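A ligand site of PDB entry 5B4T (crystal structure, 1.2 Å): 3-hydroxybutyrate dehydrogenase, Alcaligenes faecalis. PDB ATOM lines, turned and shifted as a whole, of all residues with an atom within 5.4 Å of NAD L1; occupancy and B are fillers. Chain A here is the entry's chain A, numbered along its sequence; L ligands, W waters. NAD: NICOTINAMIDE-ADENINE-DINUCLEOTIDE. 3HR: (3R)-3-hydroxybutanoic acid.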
ATOM      1  N   GLY A  11      19.083 -20.836  -3.499  1.00  0.00           N
ATOM      2  CA  GLY A  11      20.146 -19.871  -3.188  1.00  0.00           C
ATOM      3  C   GLY A  11      20.750 -20.098  -1.823  1.00  0.00           C
ATOM      4  O   GLY A  11      20.931 -19.148  -1.045  1.00  0.00           O
ATOM      5  N   SER A  12      21.180 -21.329  -1.578  1.00  0.00           N
ATOM      6  CA  SER A  12      21.699 -21.778  -0.304  1.00  0.00           C
ATOM      7  C   SER A  12      23.159 -22.198  -0.377  1.00  0.00           C
ATOM      8  O   SER A  12      23.689 -22.751   0.575  1.00  0.00           O
ATOM      9  CB  SER A  12      20.877 -22.935   0.202  1.00  0.00           C
ATOM     10  OG  SER A  12      20.664 -23.903  -0.822  1.00  0.00           O
ATOM     11  N   THR A  13      23.862 -21.717  -1.381  1.00  0.00           N
ATOM     12  CA  THR A  13      25.295 -21.945  -1.443  1.00  0.00           C
ATOM     13  C   THR A  13      26.045 -20.968  -0.580  1.00  0.00           C
ATOM     14  O   THR A  13      27.181 -21.282  -0.163  1.00  0.00           O
ATOM     15  CB  THR A  13      25.811 -21.899  -2.878  1.00  0.00           C
ATOM     16  OG1 THR A  13      25.365 -20.703  -3.505  1.00  0.00           O
ATOM     17  CG2 THR A  13      25.336 -23.121  -3.631  1.00  0.00           C
ATOM     18  N   SER A  14      25.383 -19.897  -0.178  1.00  0.00           N
ATOM     19  CA  SER A  14      26.003 -18.922   0.700  1.00  0.00           C
ATOM     20  C   SER A  14      24.931 -17.971   1.263  1.00  0.00           C
ATOM     21  O   SER A  14      23.741 -18.181   1.048  1.00  0.00           O
ATOM     22  CB  SER A  14      27.105 -18.175  -0.055  1.00  0.00           C
ATOM     23  OG  SER A  14      26.565 -17.535  -1.190  1.00  0.00           O
ATOM     24  N   GLY A  15      25.347 -17.099   2.176  1.00  0.00           N
ATOM     25  CA  GLY A  15      24.437 -16.120   2.738  1.00  0.00           C
ATOM     26  C   GLY A  15      23.338 -16.704   3.595  1.00  0.00           C
ATOM     27  O   GLY A  15      23.493 -17.707   4.317  1.00  0.00           O
ATOM     28  N   ILE A  16      22.198 -16.030   3.558  1.00  0.00           N
ATOM     29  CA  ILE A  16      21.071 -16.452   4.345  1.00  0.00           C
ATOM     30  C   ILE A  16      20.653 -17.882   4.032  1.00  0.00           C
ATOM     31  O   ILE A  16      20.302 -18.620   4.931  1.00  0.00           O
ATOM     32  CB  ILE A  16      19.916 -15.453   4.173  1.00  0.00           C
ATOM     33  CG1 ILE A  16      20.300 -14.087   4.746  1.00  0.00           C
ATOM     34  CG2 ILE A  16      18.638 -15.997   4.760  1.00  0.00           C
ATOM     35  CD1 ILE A  16      19.383 -12.965   4.308  1.00  0.00           C
ATOM     36  N   GLY A  17      20.577 -18.212   2.765  1.00  0.00           N
ATOM     37  CA  GLY A  17      20.147 -19.523   2.359  1.00  0.00           C
ATOM     38  C   GLY A  17      20.972 -20.635   2.949  1.00  0.00           C
ATOM     39  O   GLY A  17      20.439 -21.674   3.314  1.00  0.00           O
ATOM     40  N   ASN A  34      21.264 -25.243  -3.497  1.00  0.00           N
ATOM     41  CA  ASN A  34      21.114 -24.678  -4.822  1.00  0.00           C
ATOM     42  C   ASN A  34      21.845 -23.348  -4.858  1.00  0.00           C
ATOM     43  O   ASN A  34      21.924 -22.664  -3.844  1.00  0.00           O
ATOM     44  CB  ASN A  34      19.611 -24.522  -5.138  1.00  0.00           C
ATOM     45  CG  ASN A  34      19.347 -23.565  -6.264  1.00  0.00           C
ATOM     46  OD1 ASN A  34      19.057 -22.378  -6.038  1.00  0.00           O
ATOM     47  ND2 ASN A  34      19.459 -24.047  -7.490  1.00  0.00           N
ATOM     48  N   GLY A  35      22.344 -22.950  -6.006  1.00  0.00           N
ATOM     49  CA  GLY A  35      22.942 -21.639  -6.146  1.00  0.00           C
ATOM     50  C   GLY A  35      24.288 -21.714  -6.823  1.00  0.00           C
ATOM     51  O   GLY A  35      24.729 -22.775  -7.273  1.00  0.00           O
ATOM     52  N   PHE A  36      24.918 -20.564  -6.972  1.00  0.00           N
ATOM     53  CA  PHE A  36      26.167 -20.429  -7.696  1.00  0.00           C
ATOM     54  C   PHE A  36      27.325 -20.352  -6.705  1.00  0.00           C
ATOM     55  O   PHE A  36      27.137 -20.333  -5.490  1.00  0.00           O
ATOM     56  CB  PHE A  36      26.124 -19.162  -8.560  1.00  0.00           C
ATOM     57  CG  PHE A  36      25.014 -19.139  -9.567  1.00  0.00           C
ATOM     58  CD1 PHE A  36      24.262 -17.993  -9.753  1.00  0.00           C
ATOM     59  CD2 PHE A  36      24.598 -20.309 -10.213  1.00  0.00           C
ATOM     60  CE1 PHE A  36      23.306 -17.936 -10.744  1.00  0.00           C
ATOM     61  CE2 PHE A  36      23.466 -20.305 -11.017  1.00  0.00           C
ATOM     62  CZ  PHE A  36      22.857 -19.112 -11.322  1.00  0.00           C
ATOM     63  N   GLY A  37      28.537 -20.468  -7.229  1.00  0.00           N
ATOM     64  CA  GLY A  37      29.736 -20.400  -6.400  1.00  0.00           C
ATOM     65  C   GLY A  37      30.806 -21.331  -6.926  1.00  0.00           C
ATOM     66  O   GLY A  37      30.587 -22.032  -7.911  1.00  0.00           O
ATOM     67  N   ALA A  62      20.647 -24.932 -10.627  1.00  0.00           N
ATOM     68  CA  ALA A  62      19.616 -24.454 -11.516  1.00  0.00           C
ATOM     69  C   ALA A  62      19.632 -22.965 -11.445  1.00  0.00           C
ATOM     70  O   ALA A  62      19.733 -22.415 -10.339  1.00  0.00           O
ATOM     71  CB  ALA A  62      18.251 -24.982 -11.095  1.00  0.00           C
ATOM     72  N   ASP A  63      19.571 -22.296 -12.589  1.00  0.00           N
ATOM     73  CA  ASP A  63      19.462 -20.858 -12.653  1.00  0.00           C
ATOM     74  C   ASP A  63      17.987 -20.566 -12.597  1.00  0.00           C
ATOM     75  O   ASP A  63      17.237 -20.809 -13.566  1.00  0.00           O
ATOM     76  CB  ASP A  63      20.085 -20.315 -13.940  1.00  0.00           C
ATOM     77  CG  ASP A  63      19.978 -18.804 -14.053  1.00  0.00           C
ATOM     78  OD1 ASP A  63      20.622 -18.242 -14.973  1.00  0.00           O
ATOM     79  OD2 ASP A  63      19.157 -18.178 -13.384  1.00  0.00           O
ATOM     80  N   LEU A  64      17.543 -20.065 -11.467  1.00  0.00           N
ATOM     81  CA  LEU A  64      16.106 -19.941 -11.221  1.00  0.00           C
ATOM     82  C   LEU A  64      15.480 -18.718 -11.862  1.00  0.00           C
ATOM     83  O   LEU A  64      14.273 -18.502 -11.714  1.00  0.00           O
ATOM     84  CB  LEU A  64      15.872 -19.948  -9.730  1.00  0.00           C
ATOM     85  CG  LEU A  64      16.435 -21.181  -9.032  1.00  0.00           C
ATOM     86  CD1 LEU A  64      16.200 -21.082  -7.546  1.00  0.00           C
ATOM     87  CD2 LEU A  64      15.804 -22.455  -9.568  1.00  0.00           C
ATOM     88  N   SER A  65      16.238 -17.951 -12.639  1.00  0.00           N
ATOM     89  CA  SER A  65      15.647 -16.905 -13.441  1.00  0.00           C
ATOM     90  C   SER A  65      14.888 -17.450 -14.647  1.00  0.00           C
ATOM     91  O   SER A  65      14.232 -16.692 -15.348  1.00  0.00           O
ATOM     92  CB  SER A  65      16.687 -15.896 -13.896  1.00  0.00           C
ATOM     93  OG  SER A  65      17.622 -16.487 -14.770  1.00  0.00           O
ATOM     94  N   ASN A  90      14.454 -18.529  -1.391  1.00  0.00           N
ATOM     95  CA  ASN A  90      15.402 -17.556  -0.879  1.00  0.00           C
ATOM     96  C   ASN A  90      16.258 -16.824  -1.901  1.00  0.00           C
ATOM     97  O   ASN A  90      16.640 -15.681  -1.669  1.00  0.00           O
ATOM     98  CB  ASN A  90      16.274 -18.266   0.143  1.00  0.00           C
ATOM     99  CG  ASN A  90      17.482 -17.462   0.538  1.00  0.00           C
ATOM    100  OD1 ASN A  90      17.446 -16.590   1.437  1.00  0.00           O
ATOM    101  ND2 ASN A  90      18.593 -17.770  -0.105  1.00  0.00           N
ATOM    102  N   ALA A  91      16.619 -17.465  -3.002  1.00  0.00           N
ATOM    103  CA  ALA A  91      17.552 -16.871  -3.976  1.00  0.00           C
ATOM    104  C   ALA A  91      17.097 -15.477  -4.370  1.00  0.00           C
ATOM    105  O   ALA A  91      15.931 -15.258  -4.640  1.00  0.00           O
ATOM    106  CB  ALA A  91      17.615 -17.756  -5.201  1.00  0.00           C
ATOM    107  N   GLY A  92      18.012 -14.536  -4.418  1.00  0.00           N
ATOM    108  CA  GLY A  92      17.667 -13.181  -4.844  1.00  0.00           C
ATOM    109  C   GLY A  92      18.929 -12.407  -5.168  1.00  0.00           C
ATOM    110  O   GLY A  92      20.008 -12.730  -4.680  1.00  0.00           O
ATOM    111  N   ILE A  93      18.729 -11.333  -5.912  1.00  0.00           N
ATOM    112  CA  ILE A  93      19.795 -10.401  -6.259  1.00  0.00           C
ATOM    113  C   ILE A  93      19.304  -8.963  -6.035  1.00  0.00           C
ATOM    114  O   ILE A  93      18.106  -8.702  -5.866  1.00  0.00           O
ATOM    115  CB  ILE A  93      20.271 -10.585  -7.718  1.00  0.00           C
ATOM    116  CG1 ILE A  93      19.096 -10.466  -8.673  1.00  0.00           C
ATOM    117  CG2 ILE A  93      20.971 -11.934  -7.901  1.00  0.00           C
ATOM    118  CD1 ILE A  93      19.488 -10.334 -10.121  1.00  0.00           C
ATOM    119  N   LEU A 113      14.118 -13.470 -10.866  1.00  0.00           N
ATOM    120  CA  LEU A 113      14.634 -14.270  -9.763  1.00  0.00           C
ATOM    121  C   LEU A 113      13.869 -13.994  -8.489  1.00  0.00           C
ATOM    122  O   LEU A 113      13.472 -14.925  -7.778  1.00  0.00           O
ATOM    123  CB  LEU A 113      16.142 -14.036  -9.552  1.00  0.00           C
ATOM    124  CG  LEU A 113      16.736 -14.902  -8.450  1.00  0.00           C
ATOM    125  CD1 LEU A 113      16.610 -16.386  -8.806  1.00  0.00           C
ATOM    126  CD2 LEU A 113      18.171 -14.507  -8.190  1.00  0.00           C
ATOM    127  N   ASN A 114      13.738 -12.733  -8.122  1.00  0.00           N
ATOM    128  CA  ASN A 114      13.218 -12.405  -6.824  1.00  0.00           C
ATOM    129  C   ASN A 114      11.699 -12.583  -6.729  1.00  0.00           C
ATOM    130  O   ASN A 114      11.162 -12.634  -5.608  1.00  0.00           O
ATOM    131  CB  ASN A 114      13.568 -10.969  -6.438  1.00  0.00           C
ATOM    132  CG  ASN A 114      15.070 -10.741  -6.262  1.00  0.00           C
ATOM    133  OD1 ASN A 114      15.927 -11.424  -6.816  1.00  0.00           O
ATOM    134  ND2 ASN A 114      15.402  -9.703  -5.512  1.00  0.00           N
ATOM    135  N   ILE A 140      11.465 -15.745   1.382  1.00  0.00           N
ATOM    136  CA  ILE A 140      12.308 -14.735   1.964  1.00  0.00           C
ATOM    137  C   ILE A 140      12.076 -13.453   1.200  1.00  0.00           C
ATOM    138  O   ILE A 140      12.544 -13.273   0.084  1.00  0.00           O
ATOM    139  CB  ILE A 140      13.797 -15.108   1.942  1.00  0.00           C
ATOM    140  CG1 ILE A 140      14.025 -16.507   2.530  1.00  0.00           C
ATOM    141  CG2 ILE A 140      14.622 -14.062   2.697  1.00  0.00           C
ATOM    142  CD1 ILE A 140      13.466 -16.745   3.915  1.00  0.00           C
ATOM    143  N   ALA A 141      11.278 -12.573   1.797  1.00  0.00           N
ATOM    144  CA  ALA A 141      10.983 -11.276   1.241  1.00  0.00           C
ATOM    145  C   ALA A 141      11.991 -10.310   1.838  1.00  0.00           C
ATOM    146  O   ALA A 141      13.180 -10.518   1.612  1.00  0.00           O
ATOM    147  CB  ALA A 141       9.544 -10.887   1.471  1.00  0.00           C
ATOM    148  N   SER A 142      11.547  -9.259   2.506  1.00  0.00           N
ATOM    149  CA  SER A 142      12.434  -8.207   3.010  1.00  0.00           C
ATOM    150  C   SER A 142      11.543  -7.205   3.731  1.00  0.00           C
ATOM    151  O   SER A 142      10.347  -7.136   3.469  1.00  0.00           O
ATOM    152  CB  SER A 142      13.122  -7.482   1.844  1.00  0.00           C
ATOM    153  OG  SER A 142      13.835  -6.354   2.318  1.00  0.00           O
ATOM    154  N   ALA A 143      12.139  -6.352   4.565  1.00  0.00           N
ATOM    155  CA  ALA A 143      11.482  -5.122   4.922  1.00  0.00           C
ATOM    156  C   ALA A 143      10.998  -4.351   3.694  1.00  0.00           C
ATOM    157  O   ALA A 143       9.948  -3.704   3.692  1.00  0.00           O
ATOM    158  CB  ALA A 143      12.414  -4.282   5.749  1.00  0.00           C
ATOM    159  N   TYR A 155      13.740  -4.170  -6.860  1.00  0.00           N
ATOM    160  CA  TYR A 155      13.785  -5.018  -5.680  1.00  0.00           C
ATOM    161  C   TYR A 155      12.556  -4.827  -4.781  1.00  0.00           C
ATOM    162  O   TYR A 155      11.973  -5.788  -4.329  1.00  0.00           O
ATOM    163  CB  TYR A 155      15.081  -4.729  -4.927  1.00  0.00           C
ATOM    164  CG  TYR A 155      15.353  -5.633  -3.748  1.00  0.00           C
ATOM    165  CD1 TYR A 155      14.935  -5.286  -2.472  1.00  0.00           C
ATOM    166  CD2 TYR A 155      16.158  -6.754  -3.880  1.00  0.00           C
ATOM    167  CE1 TYR A 155      15.277  -6.058  -1.370  1.00  0.00           C
ATOM    168  CE2 TYR A 155      16.463  -7.554  -2.805  1.00  0.00           C
ATOM    169  CZ  TYR A 155      16.083  -7.145  -1.537  1.00  0.00           C
ATOM    170  OH  TYR A 155      16.403  -7.910  -0.434  1.00  0.00           O
ATOM    171  N   LYS A 159       9.817  -7.664  -4.061  1.00  0.00           N
ATOM    172  CA  LYS A 159       9.590  -8.100  -2.697  1.00  0.00           C
ATOM    173  C   LYS A 159       8.165  -7.835  -2.258  1.00  0.00           C
ATOM    174  O   LYS A 159       7.568  -8.651  -1.579  1.00  0.00           O
ATOM    175  CB  LYS A 159      10.589  -7.470  -1.733  1.00  0.00           C
ATOM    176  CG  LYS A 159      12.031  -7.913  -1.964  1.00  0.00           C
ATOM    177  CD  LYS A 159      12.238  -9.390  -1.766  1.00  0.00           C
ATOM    178  CE  LYS A 159      13.703  -9.787  -1.697  1.00  0.00           C
ATOM    179  NZ  LYS A 159      13.869 -11.247  -1.477  1.00  0.00           N
ATOM    180  N   PRO A 185      13.350  -9.812   6.505  1.00  0.00           N
ATOM    181  CA  PRO A 185      14.493  -9.314   7.280  1.00  0.00           C
ATOM    182  C   PRO A 185      14.831  -7.881   6.978  1.00  0.00           C
ATOM    183  O   PRO A 185      14.570  -7.388   5.885  1.00  0.00           O
ATOM    184  CB  PRO A 185      15.664 -10.222   6.833  1.00  0.00           C
ATOM    185  CG  PRO A 185      15.046 -11.342   6.064  1.00  0.00           C
ATOM    186  CD  PRO A 185      13.776 -10.775   5.478  1.00  0.00           C
ATOM    187  N   GLY A 186      15.373  -7.206   7.980  1.00  0.00           N
ATOM    188  CA  GLY A 186      16.148  -6.003   7.780  1.00  0.00           C
ATOM    189  C   GLY A 186      17.555  -6.363   7.368  1.00  0.00           C
ATOM    190  O   GLY A 186      17.782  -7.441   6.769  1.00  0.00           O
ATOM    191  N   TRP A 187      18.505  -5.457   7.564  1.00  0.00           N
ATOM    192  CA  TRP A 187      19.865  -5.690   7.086  1.00  0.00           C
ATOM    193  C   TRP A 187      20.482  -6.894   7.751  1.00  0.00           C
ATOM    194  O   TRP A 187      20.494  -6.990   8.997  1.00  0.00           O
ATOM    195  CB  TRP A 187      20.761  -4.486   7.391  1.00  0.00           C
ATOM    196  CG  TRP A 187      20.395  -3.176   6.801  1.00  0.00           C
ATOM    197  CD1 TRP A 187      20.184  -2.016   7.491  1.00  0.00           C
ATOM    198  CD2 TRP A 187      20.411  -2.821   5.426  1.00  0.00           C
ATOM    199  NE1 TRP A 187      20.078  -0.964   6.634  1.00  0.00           N
ATOM    200  CE2 TRP A 187      20.162  -1.429   5.356  1.00  0.00           C
ATOM    201  CE3 TRP A 187      20.556  -3.527   4.238  1.00  0.00           C
ATOM    202  CZ2 TRP A 187      20.203  -0.746   4.169  1.00  0.00           C
ATOM    203  CZ3 TRP A 187      20.655  -2.806   3.060  1.00  0.00           C
ATOM    204  CH2 TRP A 187      20.379  -1.460   3.030  1.00  0.00           C
ATOM    205  N   VAL A 188      21.090  -7.725   6.910  1.00  0.00           N
ATOM    206  CA  VAL A 188      21.877  -8.891   7.277  1.00  0.00           C
ATOM    207  C   VAL A 188      23.200  -8.772   6.532  1.00  0.00           C
ATOM    208  O   VAL A 188      23.202  -8.507   5.343  1.00  0.00           O
ATOM    209  CB  VAL A 188      21.195 -10.201   6.836  1.00  0.00           C
ATOM    210  CG1 VAL A 188      21.991 -11.402   7.288  1.00  0.00           C
ATOM    211  CG2 VAL A 188      19.760 -10.255   7.319  1.00  0.00           C
ATOM    212  N   ARG A 189      24.333  -8.878   7.225  1.00  0.00           N
ATOM    213  CA  ARG A 189      25.616  -8.554   6.617  1.00  0.00           C
ATOM    214  C   ARG A 189      26.144  -9.737   5.814  1.00  0.00           C
ATOM    215  O   ARG A 189      27.141 -10.379   6.168  1.00  0.00           O
ATOM    216  CB  ARG A 189      26.616  -8.082   7.639  1.00  0.00           C
ATOM    217  CG  ARG A 189      27.779  -7.342   7.014  1.00  0.00           C
ATOM    218  CD  ARG A 189      28.640  -6.694   8.064  1.00  0.00           C
ATOM    219  NE  ARG A 189      29.705  -5.954   7.410  1.00  0.00           N
ATOM    220  CZ  ARG A 189      30.474  -5.086   8.024  1.00  0.00           C
ATOM    221  NH1 ARG A 189      30.434  -4.967   9.342  1.00  0.00           N
ATOM    222  NH2 ARG A 189      31.421  -4.493   7.329  1.00  0.00           N
ATOM    223  N   THR A 190      25.543  -9.923   4.646  1.00  0.00           N
ATOM    224  CA  THR A 190      25.990 -10.879   3.625  1.00  0.00           C
ATOM    225  C   THR A 190      26.719 -10.083   2.540  1.00  0.00           C
ATOM    226  O   THR A 190      26.673  -8.877   2.517  1.00  0.00           O
ATOM    227  CB  THR A 190      24.773 -11.558   2.988  1.00  0.00           C
ATOM    228  OG1 THR A 190      24.044 -10.571   2.265  1.00  0.00           O
ATOM    229  CG2 THR A 190      23.874 -12.184   4.044  1.00  0.00           C
ATOM    230  N   PRO A 191      27.186 -10.764   1.485  1.00  0.00           N
ATOM    231  CA  PRO A 191      27.820 -10.005   0.398  1.00  0.00           C
ATOM    232  C   PRO A 191      26.886  -9.097  -0.368  1.00  0.00           C
ATOM    233  O   PRO A 191      27.324  -8.069  -0.893  1.00  0.00           O
ATOM    234  CB  PRO A 191      28.377 -11.086  -0.521  1.00  0.00           C
ATOM    235  CG  PRO A 191      28.627 -12.252   0.390  1.00  0.00           C
ATOM    236  CD  PRO A 191      27.508 -12.202   1.408  1.00  0.00           C
ATOM    237  N   LEU A 192      25.585  -9.383  -0.328  1.00  0.00           N
ATOM    238  CA  LEU A 192      24.595  -8.543  -0.955  1.00  0.00           C
ATOM    239  C   LEU A 192      24.527  -7.165  -0.298  1.00  0.00           C
ATOM    240  O   LEU A 192      24.417  -6.141  -0.964  1.00  0.00           O
ATOM    241  CB  LEU A 192      23.259  -9.254  -0.901  1.00  0.00           C
ATOM    242  CG  LEU A 192      22.069  -8.522  -1.548  1.00  0.00           C
ATOM    243  CD1 LEU A 192      21.071  -9.540  -2.088  1.00  0.00           C
ATOM    244  CD2 LEU A 192      21.413  -7.526  -0.616  1.00  0.00           C
ATOM    245  N   VAL A 193      24.782  -7.136   1.003  1.00  0.00           N
ATOM    246  CA  VAL A 193      24.818  -5.902   1.766  1.00  0.00           C
ATOM    247  C   VAL A 193      26.220  -5.324   1.855  1.00  0.00           C
ATOM    248  O   VAL A 193      26.385  -4.115   1.837  1.00  0.00           O
ATOM    249  CB  VAL A 193      24.178  -6.142   3.130  1.00  0.00           C
ATOM    250  CG1 VAL A 193      24.469  -5.036   4.112  1.00  0.00           C
ATOM    251  CG2 VAL A 193      22.666  -6.326   2.945  1.00  0.00           C
HETATM  252  PA  NAD L   1      23.669 -13.544  -1.207  1.00  0.00           P
HETATM  253  O1A NAD L   1      24.043 -12.727  -2.410  1.00  0.00           O
HETATM  254  O2A NAD L   1      24.646 -13.663  -0.094  1.00  0.00           O
HETATM  255  O5B NAD L   1      23.174 -14.994  -1.647  1.00  0.00           O
HETATM  256  C5B NAD L   1      22.348 -15.154  -2.803  1.00  0.00           C
HETATM  257  C4B NAD L   1      22.202 -16.648  -3.050  1.00  0.00           C
HETATM  258  O4B NAD L   1      21.388 -16.812  -4.211  1.00  0.00           O
HETATM  259  C3B NAD L   1      23.532 -17.321  -3.392  1.00  0.00           C
HETATM  260  O3B NAD L   1      23.475 -18.694  -2.998  1.00  0.00           O
HETATM  261  C2B NAD L   1      23.571 -17.197  -4.902  1.00  0.00           C
HETATM  262  O2B NAD L   1      24.450 -18.151  -5.531  1.00  0.00           O
HETATM  263  C1B NAD L   1      22.113 -17.522  -5.207  1.00  0.00           C
HETATM  264  N9A NAD L   1      21.652 -17.098  -6.517  1.00  0.00           N
HETATM  265  C8A NAD L   1      21.870 -15.911  -7.131  1.00  0.00           C
HETATM  266  N7A NAD L   1      21.337 -15.875  -8.364  1.00  0.00           N
HETATM  267  C5A NAD L   1      20.756 -17.078  -8.552  1.00  0.00           C
HETATM  268  C6A NAD L   1      20.038 -17.730  -9.622  1.00  0.00           C
HETATM  269  N6A NAD L   1      19.781 -17.065 -10.754  1.00  0.00           N
HETATM  270  N1A NAD L   1      19.589 -18.953  -9.385  1.00  0.00           N
HETATM  271  C2A NAD L   1      19.804 -19.630  -8.266  1.00  0.00           C
HETATM  272  N3A NAD L   1      20.482 -19.115  -7.231  1.00  0.00           N
HETATM  273  C4A NAD L   1      20.937 -17.864  -7.351  1.00  0.00           C
HETATM  274  O3  NAD L   1      22.349 -12.835  -0.658  1.00  0.00           O
HETATM  275  PN  NAD L   1      21.571 -12.913   0.727  1.00  0.00           P
HETATM  276  O1N NAD L   1      21.821 -11.579   1.405  1.00  0.00           O
HETATM  277  O2N NAD L   1      21.869 -14.175   1.431  1.00  0.00           O
HETATM  278  O5D NAD L   1      20.043 -12.879   0.229  1.00  0.00           O
HETATM  279  C5D NAD L   1      19.233 -14.045   0.230  1.00  0.00           C
HETATM  280  C4D NAD L   1      17.784 -13.579   0.154  1.00  0.00           C
HETATM  281  O4D NAD L   1      17.530 -12.765   1.305  1.00  0.00           O
HETATM  282  C3D NAD L   1      17.513 -12.718  -1.065  1.00  0.00           C
HETATM  283  O3D NAD L   1      16.180 -12.992  -1.543  1.00  0.00           O
HETATM  284  C2D NAD L   1      17.500 -11.306  -0.511  1.00  0.00           C
HETATM  285  O2D NAD L   1      16.665 -10.428  -1.238  1.00  0.00           O
HETATM  286  C1D NAD L   1      16.931 -11.577   0.858  1.00  0.00           C
HETATM  287  N1N NAD L   1      17.194 -10.517   1.834  1.00  0.00           N
HETATM  288  C2N NAD L   1      18.479 -10.227   2.185  1.00  0.00           C
HETATM  289  C3N NAD L   1      18.717  -9.268   3.153  1.00  0.00           C
HETATM  290  C7N NAD L   1      20.059  -8.820   3.560  1.00  0.00           C
HETATM  291  O7N NAD L   1      20.140  -7.806   4.263  1.00  0.00           O
HETATM  292  N7N NAD L   1      21.134  -9.502   3.186  1.00  0.00           N
HETATM  293  C4N NAD L   1      17.647  -8.696   3.831  1.00  0.00           C
HETATM  294  C5N NAD L   1      16.341  -9.061   3.499  1.00  0.00           C
HETATM  295  C6N NAD L   1      16.136  -9.967   2.480  1.00  0.00           C
HETATM  296  C1  3HR L   2      18.519  -4.623   0.479  1.00  0.00           C
HETATM  297  O1  3HR L   2      17.622  -3.747   0.548  1.00  0.00           O
HETATM  298  C2  3HR L   2      18.633  -5.736   1.486  1.00  0.00           C
HETATM  299  O2  3HR L   2      16.246  -6.218   1.622  1.00  0.00           O
HETATM  300  C3  3HR L   2      17.428  -5.968   2.389  1.00  0.00           C
HETATM  301  O3  3HR L   2      19.456  -4.544  -0.364  1.00  0.00           O
HETATM  302  C4  3HR L   2      17.193  -4.829   3.361  1.00  0.00           C
HETATM  303  O   HOH W   1      21.286 -16.636   0.468  1.00  0.00           O
HETATM  304  O   HOH W   2      20.157 -14.362 -11.853  1.00  0.00           O
HETATM  305  O   HOH W   3      22.554 -14.257 -10.322  1.00  0.00           O
HETATM  306  O   HOH W   4      26.742 -15.107  -0.449  1.00  0.00           O
HETATM  307  O   HOH W   5      26.841 -17.028  -5.578  1.00  0.00           O
HETATM  308  O   HOH W   6      22.698 -11.943  -4.609  1.00  0.00           O
HETATM  309  O   HOH W   7      24.118 -13.684  -6.156  1.00  0.00           O
HETATM  310  O   HOH W   8      26.162 -11.285  -3.140  1.00  0.00           O
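OG1 of Thr 190 is in hydrogen-bond range of O1N of NAD L1 (2.6 Å). OH of Tyr 155 sits at hydrogen-bond distance from O2D of NAD L1, 2.7 Å away. An oxygen (O3D) of NAD L1 lies within hydrogen-bond range of the backbone carbonyl oxygen (O) of Asn 90, at 2.7 Å. The backbone NH of Thr 13 sits at hydrogen-bond distance from an oxygen (O3B) of NAD L1. An oxygen (O3B) of NAD L1 is in hydrogen-bond range of the side-chain hydroxyl (OG1) of Thr 13 (2.8 Å). An oxygen (O7N) of NAD L1 is in hydrogen-bond range of the backbone NH (N) of Val 188 (2.8 Å). A nitrogen (N7N) of NAD L1 is in hydrogen-bond range of the backbone carbonyl oxygen (O) of Val 188 (3.1 Å). O2N of NAD L1 is in hydrogen-bond range of N of Ile 16. An oxygen (O2B) of NAD L1 sits at hydrogen-bond distance from the backbone NH (N) of Phe 36 (2.8 Å). O2B of NAD L1 is in hydrogen-bond range of O of Phe 36 (3.5 Å). The side-chain amino group (NZ) of Lys 159 lies within hydrogen-bond range of an oxygen (O3D) of NAD L1 (2.9 Å). A nitrogen (N6A) of NAD L1 is in hydrogen-bond range of the side-chain carboxylate of Asp 63 (2.9 Å). The backbone NH of Leu 64 lies within hydrogen-bond range of a nitrogen (N1A) of NAD L1 (3.1 Å). The backbone carbonyl oxygen of Gly 11 lies within hydrogen-bond range of an oxygen (O3B) of NAD L1 (3.2 Å). An oxygen (O2) of 3HR L2 lies within hydrogen-bond range of the side-chain hydroxyl (OH) of Tyr 155, at 2.7 Å. The side-chain hydroxyl (OG) of Ser 142 sits at hydrogen-bond distance from an oxygen (O2) of 3HR L2, at 2.5 Å.
The side-chain hydroxyl of Thr 190 sits close to the backbone NH of Leu 192 (3.2 Å). The backbone carbonyl oxygen of Gly 11 lies within hydrogen-bond range of the side-chain amide nitrogen of Asn 90 (2.9 Å). The backbone NH of Thr 13 lies within hydrogen-bond range of the backbone carbonyl oxygen of Asn 34 (3.3 Å). O of Ala 141 lies within hydrogen-bond range of NZ of Lys 159. The backbone NH (N) of Ala 143 sits at hydrogen-bond distance from the backbone carbonyl oxygen (O) of Pro 185 (3.0 Å). The side-chain amide nitrogen (ND2) of Asn 34 sits at hydrogen-bond distance from the backbone carbonyl oxygen (O) of Ala 62, at 3.3 Å. The backbone carbonyl oxygen of Asn 34 is in hydrogen-bond range of the backbone NH of Ser 12 (2.7 Å). O of Ile 93 lies within hydrogen-bond range of ND2 of Asn 114 (2.9 Å).
The backbone carbonyl oxygen (O) of Gly 186 sits close to an oxygen (O7N) of NAD L1 (3.5 Å). Residues that only touch NAD L1: Ser 12 (3.8 Å), Ser 14 (3.6 Å), Gly 15 (3.5 Å), Asn 34 (3.6 Å), Gly 35 (3.7 Å), Ala 62 (3.5 Å), Ala 91 (3.8 Å), Gly 92 (3.6 Å), Ile 93 (3.98 Å), Leu 113 (3.5 Å), Ile 140 (3.5 Å), Ala 141 (3.1 Å), Ser 142 (3.9 Å), Pro 185 (3.4 Å), Trp 187 (3.5 Å), Pro 191 (3.5 Å), Leu 192 (3.6 Å) and Val 193 (3.2 Å). Hydrophobic or aromatic side chains within 4 Å of NAD L1: Ile 16, Phe 36, Leu 64, Ala 91, Ile 93, Leu 113, Ile 140, Tyr 155, Pro 185, Val 188, Pro 191, Leu 192 and Val 193. Within 4 Å of NAD L1: Gly 11, Ser 12, Thr 13, Ser 14, Gly 15, Ile 16, Asn 34, Gly 35, Phe 36, Ala 62, Asp 63, Leu 64, Asn 90, Ala 91, Gly 92, Ile 93, Leu 113, Ile 140, Ala 141, Ser 142, Tyr 155, Lys 159, Pro 185, Gly 186, Trp 187, Val 188, Thr 190, Pro 191, Leu 192 and Val 193.
Water W4 lies within hydrogen-bond range of the side-chain hydroxyl (OG) of Ser 14 (2.5 Å) and an oxygen (O2A) of NAD L1 (2.6 Å). Water W5 bridges O2B of NAD L1 (2.6 Å) and O of Phe 36 (3.3 Å). Water W8 lies within hydrogen-bond range of an oxygen (O1A) of NAD L1 (2.7 Å) and the backbone NH (N) of Leu 192 (3.4 Å). Water W6 lies within hydrogen-bond range of an oxygen (O1A) of NAD L1 (2.7 Å) and the backbone carbonyl oxygen of Gly 92 (2.8 Å).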
